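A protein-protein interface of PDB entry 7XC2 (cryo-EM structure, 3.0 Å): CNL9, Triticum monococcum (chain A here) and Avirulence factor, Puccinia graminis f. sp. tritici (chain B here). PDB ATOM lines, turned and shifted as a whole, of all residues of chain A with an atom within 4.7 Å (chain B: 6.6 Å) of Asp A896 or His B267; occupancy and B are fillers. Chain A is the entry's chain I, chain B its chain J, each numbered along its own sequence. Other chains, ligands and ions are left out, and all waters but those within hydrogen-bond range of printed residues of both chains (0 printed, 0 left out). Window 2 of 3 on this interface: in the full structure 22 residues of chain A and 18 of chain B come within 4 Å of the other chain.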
ATOM      1  N   TRP A 835      28.277   3.562  17.547  1.00  0.00           N
ATOM      2  CA  TRP A 835      28.995   4.763  17.949  1.00  0.00           C
ATOM      3  C   TRP A 835      30.424   4.364  18.265  1.00  0.00           C
ATOM      4  O   TRP A 835      30.652   3.518  19.134  1.00  0.00           O
ATOM      5  CB  TRP A 835      28.356   5.415  19.176  1.00  0.00           C
ATOM      6  CG  TRP A 835      26.991   5.974  18.971  1.00  0.00           C
ATOM      7  CD1 TRP A 835      25.972   5.417  18.266  1.00  0.00           C
ATOM      8  CD2 TRP A 835      26.486   7.203  19.501  1.00  0.00           C
ATOM      9  NE1 TRP A 835      24.866   6.224  18.313  1.00  0.00           N
ATOM     10  CE2 TRP A 835      25.157   7.329  19.068  1.00  0.00           C
ATOM     11  CE3 TRP A 835      27.034   8.210  20.295  1.00  0.00           C
ATOM     12  CZ2 TRP A 835      24.368   8.420  19.401  1.00  0.00           C
ATOM     13  CZ3 TRP A 835      26.248   9.291  20.625  1.00  0.00           C
ATOM     14  CH2 TRP A 835      24.932   9.389  20.179  1.00  0.00           C
ATOM     15  N   VAL A 861      25.438   5.204  11.722  1.00  0.00           N
ATOM     16  CA  VAL A 861      26.753   5.217  12.346  1.00  0.00           C
ATOM     17  C   VAL A 861      27.089   6.649  12.727  1.00  0.00           C
ATOM     18  O   VAL A 861      26.900   7.570  11.926  1.00  0.00           O
ATOM     19  CB  VAL A 861      27.839   4.637  11.421  1.00  0.00           C
ATOM     20  CG1 VAL A 861      29.199   4.756  12.069  1.00  0.00           C
ATOM     21  CG2 VAL A 861      27.539   3.189  11.102  1.00  0.00           C
ATOM     22  N   VAL A 862      27.580   6.838  13.948  1.00  0.00           N
ATOM     23  CA  VAL A 862      28.002   8.138  14.451  1.00  0.00           C
ATOM     24  C   VAL A 862      29.463   8.027  14.848  1.00  0.00           C
ATOM     25  O   VAL A 862      29.816   7.204  15.700  1.00  0.00           O
ATOM     26  CB  VAL A 862      27.154   8.595  15.643  1.00  0.00           C
ATOM     27  CG1 VAL A 862      27.608   9.962  16.106  1.00  0.00           C
ATOM     28  CG2 VAL A 862      25.686   8.613  15.270  1.00  0.00           C
ATOM     29  N   VAL A 863      30.310   8.845  14.232  1.00  0.00           N
ATOM     30  CA  VAL A 863      31.748   8.786  14.447  1.00  0.00           C
ATOM     31  C   VAL A 863      32.226  10.140  14.943  1.00  0.00           C
ATOM     32  O   VAL A 863      31.559  11.162  14.761  1.00  0.00           O
ATOM     33  CB  VAL A 863      32.498   8.383  13.159  1.00  0.00           C
ATOM     34  CG1 VAL A 863      33.946   8.049  13.456  1.00  0.00           C
ATOM     35  CG2 VAL A 863      31.810   7.222  12.495  1.00  0.00           C
ATOM     36  N   ASP A 864      33.370  10.136  15.617  1.00  0.00           N
ATOM     37  CA  ASP A 864      34.092  11.353  15.949  1.00  0.00           C
ATOM     38  C   ASP A 864      35.583  11.095  15.804  1.00  0.00           C
ATOM     39  O   ASP A 864      36.075  10.027  16.182  1.00  0.00           O
ATOM     40  CB  ASP A 864      33.721  11.852  17.344  1.00  0.00           C
ATOM     41  CG  ASP A 864      33.899  10.801  18.401  1.00  0.00           C
ATOM     42  OD1 ASP A 864      35.051  10.418  18.681  1.00  0.00           O
ATOM     43  OD2 ASP A 864      32.869  10.331  18.929  1.00  0.00           O
ATOM     44  N   ILE A 894      23.672   6.220   7.590  1.00  0.00           N
ATOM     45  CA  ILE A 894      23.955   7.646   7.669  1.00  0.00           C
ATOM     46  C   ILE A 894      25.179   7.859   8.541  1.00  0.00           C
ATOM     47  O   ILE A 894      25.393   7.133   9.521  1.00  0.00           O
ATOM     48  CB  ILE A 894      22.740   8.410   8.221  1.00  0.00           C
ATOM     49  CG1 ILE A 894      21.462   7.868   7.587  1.00  0.00           C
ATOM     50  CG2 ILE A 894      22.882   9.893   7.953  1.00  0.00           C
ATOM     51  CD1 ILE A 894      20.205   8.494   8.127  1.00  0.00           C
ATOM     52  N   LEU A 895      25.988   8.851   8.190  1.00  0.00           N
ATOM     53  CA  LEU A 895      27.211   9.148   8.916  1.00  0.00           C
ATOM     54  C   LEU A 895      27.128  10.484   9.636  1.00  0.00           C
ATOM     55  O   LEU A 895      26.324  11.358   9.296  1.00  0.00           O
ATOM     56  CB  LEU A 895      28.422   9.164   7.984  1.00  0.00           C
ATOM     57  CG  LEU A 895      28.907   7.816   7.479  1.00  0.00           C
ATOM     58  CD1 LEU A 895      30.173   8.024   6.680  1.00  0.00           C
ATOM     59  CD2 LEU A 895      29.146   6.881   8.646  1.00  0.00           C
ATOM     60  N   ASP A 896      27.996  10.623  10.638  1.00  0.00           N
ATOM     61  CA  ASP A 896      28.212  11.864  11.368  1.00  0.00           C
ATOM     62  C   ASP A 896      29.634  11.843  11.902  1.00  0.00           C
ATOM     63  O   ASP A 896      29.982  10.951  12.679  1.00  0.00           O
ATOM     64  CB  ASP A 896      27.223  12.011  12.523  1.00  0.00           C
ATOM     65  CG  ASP A 896      25.818  12.286  12.052  1.00  0.00           C
ATOM     66  OD1 ASP A 896      25.643  13.222  11.250  1.00  0.00           O
ATOM     67  OD2 ASP A 896      24.897  11.562  12.480  1.00  0.00           O
ATOM     68  N   ILE A 897      30.453  12.809  11.490  1.00  0.00           N
ATOM     69  CA  ILE A 897      31.868  12.791  11.858  1.00  0.00           C
ATOM     70  C   ILE A 897      32.123  13.614  13.112  1.00  0.00           C
ATOM     71  O   ILE A 897      32.967  13.248  13.935  1.00  0.00           O
ATOM     72  CB  ILE A 897      32.746  13.258  10.682  1.00  0.00           C
ATOM     73  CG1 ILE A 897      32.676  12.267   9.524  1.00  0.00           C
ATOM     74  CG2 ILE A 897      34.198  13.448  11.157  1.00  0.00           C
ATOM     75  CD1 ILE A 897      33.304  12.795   8.236  1.00  0.00           C
ATOM     76  N   TRP A 898      31.446  14.750  13.252  1.00  0.00           N
ATOM     77  CA  TRP A 898      31.564  15.555  14.465  1.00  0.00           C
ATOM     78  C   TRP A 898      33.004  15.967  14.781  1.00  0.00           C
ATOM     79  O   TRP A 898      33.876  15.940  13.916  1.00  0.00           O
ATOM     80  CB  TRP A 898      30.967  14.799  15.657  1.00  0.00           C
ATOM     81  CG  TRP A 898      29.476  14.727  15.613  1.00  0.00           C
ATOM     82  CD1 TRP A 898      28.706  13.619  15.428  1.00  0.00           C
ATOM     83  CD2 TRP A 898      28.571  15.820  15.781  1.00  0.00           C
ATOM     84  NE1 TRP A 898      27.376  13.958  15.452  1.00  0.00           N
ATOM     85  CE2 TRP A 898      27.267  15.306  15.674  1.00  0.00           C
ATOM     86  CE3 TRP A 898      28.741  17.189  16.009  1.00  0.00           C
ATOM     87  CZ2 TRP A 898      26.136  16.111  15.785  1.00  0.00           C
ATOM     88  CZ3 TRP A 898      27.622  17.985  16.120  1.00  0.00           C
ATOM     89  CH2 TRP A 898      26.335  17.446  16.008  1.00  0.00           C
ATOM     90  N   PHE B 262      26.700  15.531  27.628  1.00  0.00           N
ATOM     91  CA  PHE B 262      26.588  16.242  26.360  1.00  0.00           C
ATOM     92  C   PHE B 262      27.894  16.935  26.006  1.00  0.00           C
ATOM     93  O   PHE B 262      28.303  16.952  24.840  1.00  0.00           O
ATOM     94  CB  PHE B 262      25.458  17.263  26.416  1.00  0.00           C
ATOM     95  CG  PHE B 262      25.614  18.385  25.435  1.00  0.00           C
ATOM     96  CD1 PHE B 262      25.231  18.225  24.121  1.00  0.00           C
ATOM     97  CD2 PHE B 262      26.146  19.599  25.826  1.00  0.00           C
ATOM     98  CE1 PHE B 262      25.373  19.249  23.215  1.00  0.00           C
ATOM     99  CE2 PHE B 262      26.292  20.625  24.922  1.00  0.00           C
ATOM    100  CZ  PHE B 262      25.904  20.450  23.616  1.00  0.00           C
ATOM    101  N   SER B 265      30.368  14.253  24.458  1.00  0.00           N
ATOM    102  CA  SER B 265      29.953  13.721  23.161  1.00  0.00           C
ATOM    103  C   SER B 265      28.726  14.496  22.707  1.00  0.00           C
ATOM    104  O   SER B 265      27.603  14.202  23.152  1.00  0.00           O
ATOM    105  CB  SER B 265      29.658  12.231  23.234  1.00  0.00           C
ATOM    106  OG  SER B 265      28.583  11.978  24.114  1.00  0.00           O
ATOM    107  N   PRO B 266      28.890  15.476  21.820  1.00  0.00           N
ATOM    108  CA  PRO B 266      27.779  16.396  21.543  1.00  0.00           C
ATOM    109  C   PRO B 266      26.625  15.759  20.802  1.00  0.00           C
ATOM    110  O   PRO B 266      25.493  16.243  20.921  1.00  0.00           O
ATOM    111  CB  PRO B 266      28.443  17.494  20.707  1.00  0.00           C
ATOM    112  CG  PRO B 266      29.580  16.809  20.052  1.00  0.00           C
ATOM    113  CD  PRO B 266      30.085  15.798  21.030  1.00  0.00           C
ATOM    114  N   HIS B 267      26.865  14.686  20.050  1.00  0.00           N
ATOM    115  CA  HIS B 267      25.804  14.124  19.225  1.00  0.00           C
ATOM    116  C   HIS B 267      24.590  13.694  20.033  1.00  0.00           C
ATOM    117  O   HIS B 267      23.523  13.483  19.446  1.00  0.00           O
ATOM    118  CB  HIS B 267      26.324  12.934  18.429  1.00  0.00           C
ATOM    119  CG  HIS B 267      25.319  12.378  17.472  1.00  0.00           C
ATOM    120  ND1 HIS B 267      24.749  13.135  16.472  1.00  0.00           N
ATOM    121  CD2 HIS B 267      24.757  11.151  17.382  1.00  0.00           C
ATOM    122  CE1 HIS B 267      23.894  12.391  15.794  1.00  0.00           C
ATOM    123  NE2 HIS B 267      23.881  11.184  16.326  1.00  0.00           N
ATOM    124  N   ARG B 268      24.722  13.567  21.354  1.00  0.00           N
ATOM    125  CA  ARG B 268      23.570  13.259  22.189  1.00  0.00           C
ATOM    126  C   ARG B 268      22.429  14.230  21.944  1.00  0.00           C
ATOM    127  O   ARG B 268      21.259  13.852  22.057  1.00  0.00           O
ATOM    128  CB  ARG B 268      23.968  13.290  23.660  1.00  0.00           C
ATOM    129  CG  ARG B 268      24.847  12.144  24.082  1.00  0.00           C
ATOM    130  CD  ARG B 268      24.821  11.978  25.581  1.00  0.00           C
ATOM    131  NE  ARG B 268      24.975  10.580  25.959  1.00  0.00           N
ATOM    132  CZ  ARG B 268      24.597  10.080  27.128  1.00  0.00           C
ATOM    133  NH1 ARG B 268      24.040  10.868  28.035  1.00  0.00           N
ATOM    134  NH2 ARG B 268      24.775   8.795  27.386  1.00  0.00           N
ATOM    135  N   LYS B 269      22.746  15.478  21.601  1.00  0.00           N
ATOM    136  CA  LYS B 269      21.697  16.458  21.355  1.00  0.00           C
ATOM    137  C   LYS B 269      20.809  16.052  20.188  1.00  0.00           C
ATOM    138  O   LYS B 269      19.600  16.301  20.215  1.00  0.00           O
ATOM    139  CB  LYS B 269      22.318  17.827  21.100  1.00  0.00           C
ATOM    140  CG  LYS B 269      21.324  18.907  20.733  1.00  0.00           C
ATOM    141  CD  LYS B 269      22.012  20.252  20.652  1.00  0.00           C
ATOM    142  CE  LYS B 269      21.017  21.381  20.506  1.00  0.00           C
ATOM    143  NZ  LYS B 269      21.693  22.704  20.583  1.00  0.00           N
ATOM    144  N   ILE B 270      21.380  15.415  19.166  1.00  0.00           N
ATOM    145  CA  ILE B 270      20.588  15.036  18.001  1.00  0.00           C
ATOM    146  C   ILE B 270      19.664  13.874  18.334  1.00  0.00           C
ATOM    147  O   ILE B 270      18.501  13.853  17.920  1.00  0.00           O
ATOM    148  CB  ILE B 270      21.513  14.705  16.820  1.00  0.00           C
ATOM    149  CG1 ILE B 270      22.378  15.915  16.474  1.00  0.00           C
ATOM    150  CG2 ILE B 270      20.701  14.276  15.619  1.00  0.00           C
ATOM    151  CD1 ILE B 270      21.595  17.194  16.322  1.00  0.00           C
ATOM    152  N   ILE B 271      20.161  12.896  19.080  1.00  0.00           N
ATOM    153  CA  ILE B 271      19.355  11.762  19.520  1.00  0.00           C
ATOM    154  C   ILE B 271      19.229  11.832  21.036  1.00  0.00           C
ATOM    155  O   ILE B 271      19.951  11.123  21.752  1.00  0.00           O
ATOM    156  CB  ILE B 271      19.971  10.429  19.079  1.00  0.00           C
ATOM    157  CG1 ILE B 271      20.437  10.523  17.628  1.00  0.00           C
ATOM    158  CG2 ILE B 271      18.970   9.305  19.247  1.00  0.00           C
ATOM    159  CD1 ILE B 271      21.278   9.355  17.191  1.00  0.00           C
ATOM    160  N   PRO B 272      18.342  12.662  21.566  1.00  0.00           N
ATOM    161  CA  PRO B 272      18.310  12.882  23.011  1.00  0.00           C
ATOM    162  C   PRO B 272      17.593  11.769  23.749  1.00  0.00           C
ATOM    163  O   PRO B 272      16.668  11.137  23.235  1.00  0.00           O
ATOM    164  CB  PRO B 272      17.540  14.204  23.150  1.00  0.00           C
ATOM    165  CG  PRO B 272      17.319  14.703  21.738  1.00  0.00           C
ATOM    166  CD  PRO B 272      17.362  13.502  20.871  1.00  0.00           C
ATOM    167  N   LEU B 276      17.603  14.629  28.593  1.00  0.00           N
ATOM    168  CA  LEU B 276      18.003  15.667  27.657  1.00  0.00           C
ATOM    169  C   LEU B 276      16.786  16.300  26.995  1.00  0.00           C
ATOM    170  O   LEU B 276      16.780  17.505  26.713  1.00  0.00           O
ATOM    171  CB  LEU B 276      18.963  15.100  26.621  1.00  0.00           C
ATOM    172  CG  LEU B 276      19.914  16.141  26.037  1.00  0.00           C
ATOM    173  CD1 LEU B 276      20.647  16.897  27.125  1.00  0.00           C
ATOM    174  CD2 LEU B 276      20.911  15.470  25.127  1.00  0.00           C
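Printed residues of chain B within 4 Å of Trp A835: His B267 and Ile B271. Of the printed residues of chain B, Val A862 touches His B267. Val A863 touches none of the printed residues of chain B. Asp A896 touches one residue of chain B. Of the printed residues of chain B, Trp A898 touches His B267 (2.9 Å) and Ile B270 (3.8 Å). Printed residues of chain A within 4 Å of Ile B270: Trp A898. Printed residues of chain A within 4 Å of Ile B271: Trp A835 (3.9 Å). The nearest printed residue of chain A that does not touch His B267 is Val A861 (6.4 Å). The nearest printed residue of chain A that does not touch Ile B270 is Asp A896 (5.9 Å).
The indole nitrogen (NE1) of Trp A898 lies within hydrogen-bond range of a ring nitrogen (ND1) of His B267.
Hydrophobic or aromatic side chains of chain B within 4 Å of the printed part of chain A: His B267, Ile B270 and Ile B271. Among the printed residues, 6 pairs touch across the chains. Among the printed residues, no Asp or Glu carboxylate lies within 4 Å of a Lys or Arg side-chain nitrogen of the other chain.
His B267 touches Trp A835. Trp A835 touches Ile B271 (CZ2 to CD1, 3.9 Å). CG2 of Val A862 touches NE2 of His B267, at 3.3 Å. His B267 touches Asp A896. Trp A898 touches Ile B270.
The backbone carbonyl oxygen of Val A861 is in hydrogen-bond range of the backbone NH of Asp A896. The backbone NH (N) of Val A863 lies within hydrogen-bond range of the backbone carbonyl oxygen (O) of Asp A896.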
